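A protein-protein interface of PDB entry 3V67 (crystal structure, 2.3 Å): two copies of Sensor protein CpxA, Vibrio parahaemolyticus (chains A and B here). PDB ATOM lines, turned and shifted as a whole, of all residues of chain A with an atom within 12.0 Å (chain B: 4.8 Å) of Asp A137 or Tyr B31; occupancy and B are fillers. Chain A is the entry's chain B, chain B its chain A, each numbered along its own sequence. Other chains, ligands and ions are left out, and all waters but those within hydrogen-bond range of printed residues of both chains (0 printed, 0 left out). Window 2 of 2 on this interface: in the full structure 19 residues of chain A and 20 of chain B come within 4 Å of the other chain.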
ATOM      1  N   LEU A 132       3.632  28.765   7.591  1.00  0.00           N
ATOM      2  CA  LEU A 132       4.754  27.911   7.979  1.00  0.00           C
ATOM      3  C   LEU A 132       4.935  26.686   7.072  1.00  0.00           C
ATOM      4  O   LEU A 132       4.023  25.876   6.894  1.00  0.00           O
ATOM      5  CB  LEU A 132       4.644  27.520   9.464  1.00  0.00           C
ATOM      6  CG  LEU A 132       4.661  26.066   9.953  1.00  0.00           C
ATOM      7  CD1 LEU A 132       6.049  25.628  10.416  1.00  0.00           C
ATOM      8  CD2 LEU A 132       3.641  25.892  11.067  1.00  0.00           C
ATOM      9  N   LEU A 133       6.121  26.592   6.477  1.00  0.00           N
ATOM     10  CA  LEU A 133       6.505  25.485   5.605  1.00  0.00           C
ATOM     11  C   LEU A 133       8.007  25.267   5.750  1.00  0.00           C
ATOM     12  O   LEU A 133       8.664  25.995   6.496  1.00  0.00           O
ATOM     13  CB  LEU A 133       6.147  25.797   4.151  1.00  0.00           C
ATOM     14  CG  LEU A 133       6.074  27.281   3.779  1.00  0.00           C
ATOM     15  CD1 LEU A 133       7.451  27.946   3.726  1.00  0.00           C
ATOM     16  CD2 LEU A 133       5.325  27.475   2.471  1.00  0.00           C
ATOM     17  N   ARG A 134       8.563  24.288   5.039  1.00  0.00           N
ATOM     18  CA  ARG A 134       9.988  24.003   5.188  1.00  0.00           C
ATOM     19  C   ARG A 134      10.636  23.293   4.002  1.00  0.00           C
ATOM     20  O   ARG A 134       9.959  22.864   3.066  1.00  0.00           O
ATOM     21  CB  ARG A 134      10.223  23.197   6.468  1.00  0.00           C
ATOM     22  CG  ARG A 134      11.583  23.406   7.112  1.00  0.00           C
ATOM     23  CD  ARG A 134      11.479  23.288   8.615  1.00  0.00           C
ATOM     24  NE  ARG A 134      12.474  22.372   9.157  1.00  0.00           N
ATOM     25  CZ  ARG A 134      12.400  21.049   9.056  1.00  0.00           C
ATOM     26  NH1 ARG A 134      11.373  20.486   8.431  1.00  0.00           N
ATOM     27  NH2 ARG A 134      13.347  20.286   9.580  1.00  0.00           N
ATOM     28  N   LEU A 135      11.962  23.186   4.064  1.00  0.00           N
ATOM     29  CA  LEU A 135      12.756  22.510   3.049  1.00  0.00           C
ATOM     30  C   LEU A 135      13.832  21.609   3.675  1.00  0.00           C
ATOM     31  O   LEU A 135      14.687  21.076   2.971  1.00  0.00           O
ATOM     32  CB  LEU A 135      13.389  23.541   2.109  1.00  0.00           C
ATOM     33  CG  LEU A 135      13.859  23.073   0.729  1.00  0.00           C
ATOM     34  CD1 LEU A 135      13.247  23.928  -0.376  1.00  0.00           C
ATOM     35  CD2 LEU A 135      15.377  23.082   0.637  1.00  0.00           C
ATOM     36  N   PHE A 136      13.791  21.426   4.994  1.00  0.00           N
ATOM     37  CA  PHE A 136      14.745  20.518   5.640  1.00  0.00           C
ATOM     38  C   PHE A 136      14.153  19.113   5.740  1.00  0.00           C
ATOM     39  O   PHE A 136      13.610  18.725   6.775  1.00  0.00           O
ATOM     40  CB  PHE A 136      15.157  21.008   7.031  1.00  0.00           C
ATOM     41  CG  PHE A 136      15.560  22.455   7.079  1.00  0.00           C
ATOM     42  CD1 PHE A 136      15.407  23.188   8.245  1.00  0.00           C
ATOM     43  CD2 PHE A 136      16.097  23.081   5.966  1.00  0.00           C
ATOM     44  CE1 PHE A 136      15.773  24.522   8.296  1.00  0.00           C
ATOM     45  CE2 PHE A 136      16.460  24.412   6.012  1.00  0.00           C
ATOM     46  CZ  PHE A 136      16.298  25.133   7.177  1.00  0.00           C
ATOM     47  N   ASP A 137      14.261  18.351   4.656  1.00  0.00           N
ATOM     48  CA  ASP A 137      13.676  17.016   4.601  1.00  0.00           C
ATOM     49  C   ASP A 137      14.467  16.075   3.698  1.00  0.00           C
ATOM     50  O   ASP A 137      14.321  14.854   3.782  1.00  0.00           O
ATOM     51  CB  ASP A 137      12.218  17.092   4.140  1.00  0.00           C
ATOM     52  CG  ASP A 137      12.011  18.088   3.012  1.00  0.00           C
ATOM     53  OD1 ASP A 137      10.986  18.804   3.030  1.00  0.00           O
ATOM     54  OD2 ASP A 137      12.869  18.158   2.106  1.00  0.00           O
ATOM     55  N   THR B  23       8.988  20.512  -2.987  1.00  0.00           N
ATOM     56  CA  THR B  23       9.570  19.640  -1.968  1.00  0.00           C
ATOM     57  C   THR B  23       9.541  18.180  -2.409  1.00  0.00           C
ATOM     58  O   THR B  23      10.355  17.377  -1.963  1.00  0.00           O
ATOM     59  CB  THR B  23       8.888  19.770  -0.582  1.00  0.00           C
ATOM     60  OG1 THR B  23       7.911  18.737  -0.419  1.00  0.00           O
ATOM     61  CG2 THR B  23       8.238  21.130  -0.409  1.00  0.00           C
ATOM     62  N   ILE B  27      12.908  16.116  -2.429  1.00  0.00           N
ATOM     63  CA  ILE B  27      13.045  14.830  -1.752  1.00  0.00           C
ATOM     64  C   ILE B  27      13.507  13.762  -2.740  1.00  0.00           C
ATOM     65  O   ILE B  27      14.344  12.914  -2.414  1.00  0.00           O
ATOM     66  CB  ILE B  27      11.720  14.402  -1.078  1.00  0.00           C
ATOM     67  CG1 ILE B  27      11.441  15.275   0.149  1.00  0.00           C
ATOM     68  CG2 ILE B  27      11.762  12.939  -0.673  1.00  0.00           C
ATOM     69  CD1 ILE B  27      10.222  14.844   0.948  1.00  0.00           C
ATOM     70  N   GLN B  28      12.964  13.823  -3.952  1.00  0.00           N
ATOM     71  CA  GLN B  28      13.358  12.918  -5.025  1.00  0.00           C
ATOM     72  C   GLN B  28      14.841  13.039  -5.346  1.00  0.00           C
ATOM     73  O   GLN B  28      15.533  12.038  -5.515  1.00  0.00           O
ATOM     74  CB  GLN B  28      12.533  13.190  -6.285  1.00  0.00           C
ATOM     75  CG  GLN B  28      11.361  12.255  -6.477  1.00  0.00           C
ATOM     76  CD  GLN B  28      10.580  12.551  -7.737  1.00  0.00           C
ATOM     77  OE1 GLN B  28       9.679  11.801  -8.111  1.00  0.00           O
ATOM     78  NE2 GLN B  28      10.927  13.644  -8.405  1.00  0.00           N
ATOM     79  N   ASN B  29      15.326  14.272  -5.431  1.00  0.00           N
ATOM     80  CA  ASN B  29      16.724  14.511  -5.768  1.00  0.00           C
ATOM     81  C   ASN B  29      17.692  14.220  -4.627  1.00  0.00           C
ATOM     82  O   ASN B  29      18.826  13.801  -4.860  1.00  0.00           O
ATOM     83  CB  ASN B  29      16.924  15.939  -6.283  1.00  0.00           C
ATOM     84  CG  ASN B  29      16.937  16.010  -7.794  1.00  0.00           C
ATOM     85  OD1 ASN B  29      17.407  15.089  -8.464  1.00  0.00           O
ATOM     86  ND2 ASN B  29      16.418  17.104  -8.343  1.00  0.00           N
ATOM     87  N   LYS B  30      17.243  14.440  -3.396  1.00  0.00           N
ATOM     88  CA  LYS B  30      18.085  14.203  -2.231  1.00  0.00           C
ATOM     89  C   LYS B  30      18.395  12.722  -2.046  1.00  0.00           C
ATOM     90  O   LYS B  30      19.530  12.346  -1.748  1.00  0.00           O
ATOM     91  CB  LYS B  30      17.429  14.753  -0.966  1.00  0.00           C
ATOM     92  CG  LYS B  30      18.171  14.376   0.302  1.00  0.00           C
ATOM     93  CD  LYS B  30      17.668  15.148   1.505  1.00  0.00           C
ATOM     94  CE  LYS B  30      18.483  14.803   2.740  1.00  0.00           C
ATOM     95  NZ  LYS B  30      18.095  15.634   3.910  1.00  0.00           N
ATOM     96  N   TYR B  31      17.382  11.884  -2.231  1.00  0.00           N
ATOM     97  CA  TYR B  31      17.525  10.455  -1.986  1.00  0.00           C
ATOM     98  C   TYR B  31      17.608   9.645  -3.273  1.00  0.00           C
ATOM     99  O   TYR B  31      17.256   8.466  -3.293  1.00  0.00           O
ATOM    100  CB  TYR B  31      16.368   9.954  -1.124  1.00  0.00           C
ATOM    101  CG  TYR B  31      16.284  10.650   0.211  1.00  0.00           C
ATOM    102  CD1 TYR B  31      15.443  11.739   0.398  1.00  0.00           C
ATOM    103  CD2 TYR B  31      17.059  10.230   1.280  1.00  0.00           C
ATOM    104  CE1 TYR B  31      15.370  12.383   1.619  1.00  0.00           C
ATOM    105  CE2 TYR B  31      16.995  10.865   2.503  1.00  0.00           C
ATOM    106  CZ  TYR B  31      16.149  11.941   2.669  1.00  0.00           C
ATOM    107  OH  TYR B  31      16.086  12.575   3.889  1.00  0.00           O
ATOM    108  N   SER B  32      18.081  10.279  -4.340  1.00  0.00           N
ATOM    109  CA  SER B  32      18.207   9.613  -5.632  1.00  0.00           C
ATOM    110  C   SER B  32      19.238   8.490  -5.571  1.00  0.00           C
ATOM    111  O   SER B  32      19.179   7.532  -6.343  1.00  0.00           O
ATOM    112  CB  SER B  32      18.586  10.620  -6.720  1.00  0.00           C
ATOM    113  OG  SER B  32      19.826  11.243  -6.430  1.00  0.00           O
ATOM    114  N   LYS B  33      20.180   8.615  -4.643  1.00  0.00           N
ATOM    115  CA  LYS B  33      21.230   7.620  -4.480  1.00  0.00           C
ATOM    116  C   LYS B  33      20.742   6.388  -3.724  1.00  0.00           C
ATOM    117  O   LYS B  33      21.244   5.283  -3.936  1.00  0.00           O
ATOM    118  CB  LYS B  33      22.429   8.233  -3.756  1.00  0.00           C
ATOM    119  CG  LYS B  33      22.052   9.094  -2.556  1.00  0.00           C
ATOM    120  CD  LYS B  33      23.245   9.308  -1.639  1.00  0.00           C
ATOM    121  CE  LYS B  33      24.450   9.829  -2.406  1.00  0.00           C
ATOM    122  NZ  LYS B  33      24.801  11.220  -2.009  1.00  0.00           N
ATOM    123  N   GLU B  34      19.762   6.577  -2.847  1.00  0.00           N
ATOM    124  CA  GLU B  34      19.302   5.501  -1.973  1.00  0.00           C
ATOM    125  C   GLU B  34      18.433   4.475  -2.704  1.00  0.00           C
ATOM    126  O   GLU B  34      17.518   4.836  -3.444  1.00  0.00           O
ATOM    127  CB  GLU B  34      18.561   6.071  -0.760  1.00  0.00           C
ATOM    128  CG  GLU B  34      18.197   5.027   0.278  1.00  0.00           C
ATOM    129  CD  GLU B  34      19.396   4.230   0.748  1.00  0.00           C
ATOM    130  OE1 GLU B  34      19.313   2.984   0.753  1.00  0.00           O
ATOM    131  OE2 GLU B  34      20.420   4.845   1.114  1.00  0.00           O
ATOM    132  N   ILE B  40      14.793   5.406   3.151  1.00  0.00           N
ATOM    133  CA  ILE B  40      14.318   6.714   2.719  1.00  0.00           C
ATOM    134  C   ILE B  40      13.200   7.229   3.620  1.00  0.00           C
ATOM    135  O   ILE B  40      13.253   8.362   4.096  1.00  0.00           O
ATOM    136  CB  ILE B  40      13.803   6.690   1.266  1.00  0.00           C
ATOM    137  CG1 ILE B  40      14.932   6.342   0.299  1.00  0.00           C
ATOM    138  CG2 ILE B  40      13.196   8.033   0.900  1.00  0.00           C
ATOM    139  CD1 ILE B  40      14.524   6.406  -1.164  1.00  0.00           C
ATOM    140  N   ARG B  43      14.533   8.091   7.111  1.00  0.00           N
ATOM    141  CA  ARG B  43      15.260   9.360   7.073  1.00  0.00           C
ATOM    142  C   ARG B  43      14.338  10.572   6.954  1.00  0.00           C
ATOM    143  O   ARG B  43      14.463  11.531   7.714  1.00  0.00           O
ATOM    144  CB  ARG B  43      16.256   9.377   5.910  1.00  0.00           C
ATOM    145  CG  ARG B  43      17.648   8.864   6.236  1.00  0.00           C
ATOM    146  CD  ARG B  43      18.554   8.992   5.020  1.00  0.00           C
ATOM    147  NE  ARG B  43      19.915   8.536   5.276  1.00  0.00           N
ATOM    148  CZ  ARG B  43      20.846   8.407   4.335  1.00  0.00           C
ATOM    149  NH1 ARG B  43      20.558   8.696   3.071  1.00  0.00           N
ATOM    150  NH2 ARG B  43      22.062   7.984   4.653  1.00  0.00           N
ATOM    151  N   VAL B  44      13.427  10.524   5.987  1.00  0.00           N
ATOM    152  CA  VAL B  44      12.498  11.620   5.734  1.00  0.00           C
ATOM    153  C   VAL B  44      11.661  11.949   6.958  1.00  0.00           C
ATOM    154  O   VAL B  44      11.540  13.108   7.349  1.00  0.00           O
ATOM    155  CB  VAL B  44      11.558  11.307   4.541  1.00  0.00           C
ATOM    156  CG1 VAL B  44      10.312  12.179   4.589  1.00  0.00           C
ATOM    157  CG2 VAL B  44      12.292  11.493   3.223  1.00  0.00           C
ATOM    158  N   ASN B  47      13.120  13.778  10.485  1.00  0.00           N
ATOM    159  CA  ASN B  47      13.348  15.197  10.736  1.00  0.00           C
ATOM    160  C   ASN B  47      12.306  15.880  11.625  1.00  0.00           C
ATOM    161  O   ASN B  47      12.464  17.049  11.980  1.00  0.00           O
ATOM    162  CB  ASN B  47      13.542  15.966   9.426  1.00  0.00           C
ATOM    163  CG  ASN B  47      15.009  16.170   9.087  1.00  0.00           C
ATOM    164  OD1 ASN B  47      15.868  16.153   9.970  1.00  0.00           O
ATOM    165  ND2 ASN B  47      15.302  16.366   7.807  1.00  0.00           N
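Of the printed residues of chain B, Asp A137 touches Ile B27 (3.8 Å), Lys B30 (3.7 Å), Tyr B31 (2.9 Å), Val B44 (3.97 Å) and Asn B47 (3.7 Å). No residue of chain A comes within 4 Å of Thr B23. Ile B27 touches one residue of chain A. Lys B30 touches just one residue of chain A: Asp A137 (3.7 Å). No residue of chain A comes within 4 Å of Ser B32. No residue of chain A comes within 4 Å of Lys B33. Ile B40 touches none of the printed residues of chain A. Of the printed residues of chain B, Phe A136 touches Asn B47 (3.1 Å). Asn B29 touches none of the printed residues of chain A. Leu A135 touches none of the printed residues of chain B. The nearest residue of chain B that does not touch Asp A137 is Thr B23 (4.3 Å).
The backbone carbonyl oxygen of Asp A137 sits at hydrogen-bond distance from the side-chain hydroxyl of Tyr B31, 2.9 Å away. The side-chain amide nitrogen (ND2) of Asn B47 sits at hydrogen-bond distance from the backbone carbonyl oxygen (O) of Phe A136 (3.1 Å).
No position is printed for both chains. Of the 6 pairs that touch across the chains among the printed residues, none has its exchanged pair printed and touching as well.
The backbone carbonyl oxygen (O) of Phe A136 sits close to the guanidinium group (NH2) of Arg A134 (3.2 Å).
Of the 13 printed residues of chain B, 5 touch a printed residue of chain A. Hydrophobic or aromatic side chains of chain B within 4 Å of the printed part of chain A: Ile B27, Tyr B31 and Val B44.
OD2 of Asp A137 touches CG1 of Ile B27, at 3.8 Å. NZ of Lys B30 touches C of Asp A137, at 3.7 Å. Asp A137 touches Val B44 (O to CG2, 3.97 Å). Asp A137 touches Asn B47 (CA to ND2, 3.7 Å).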
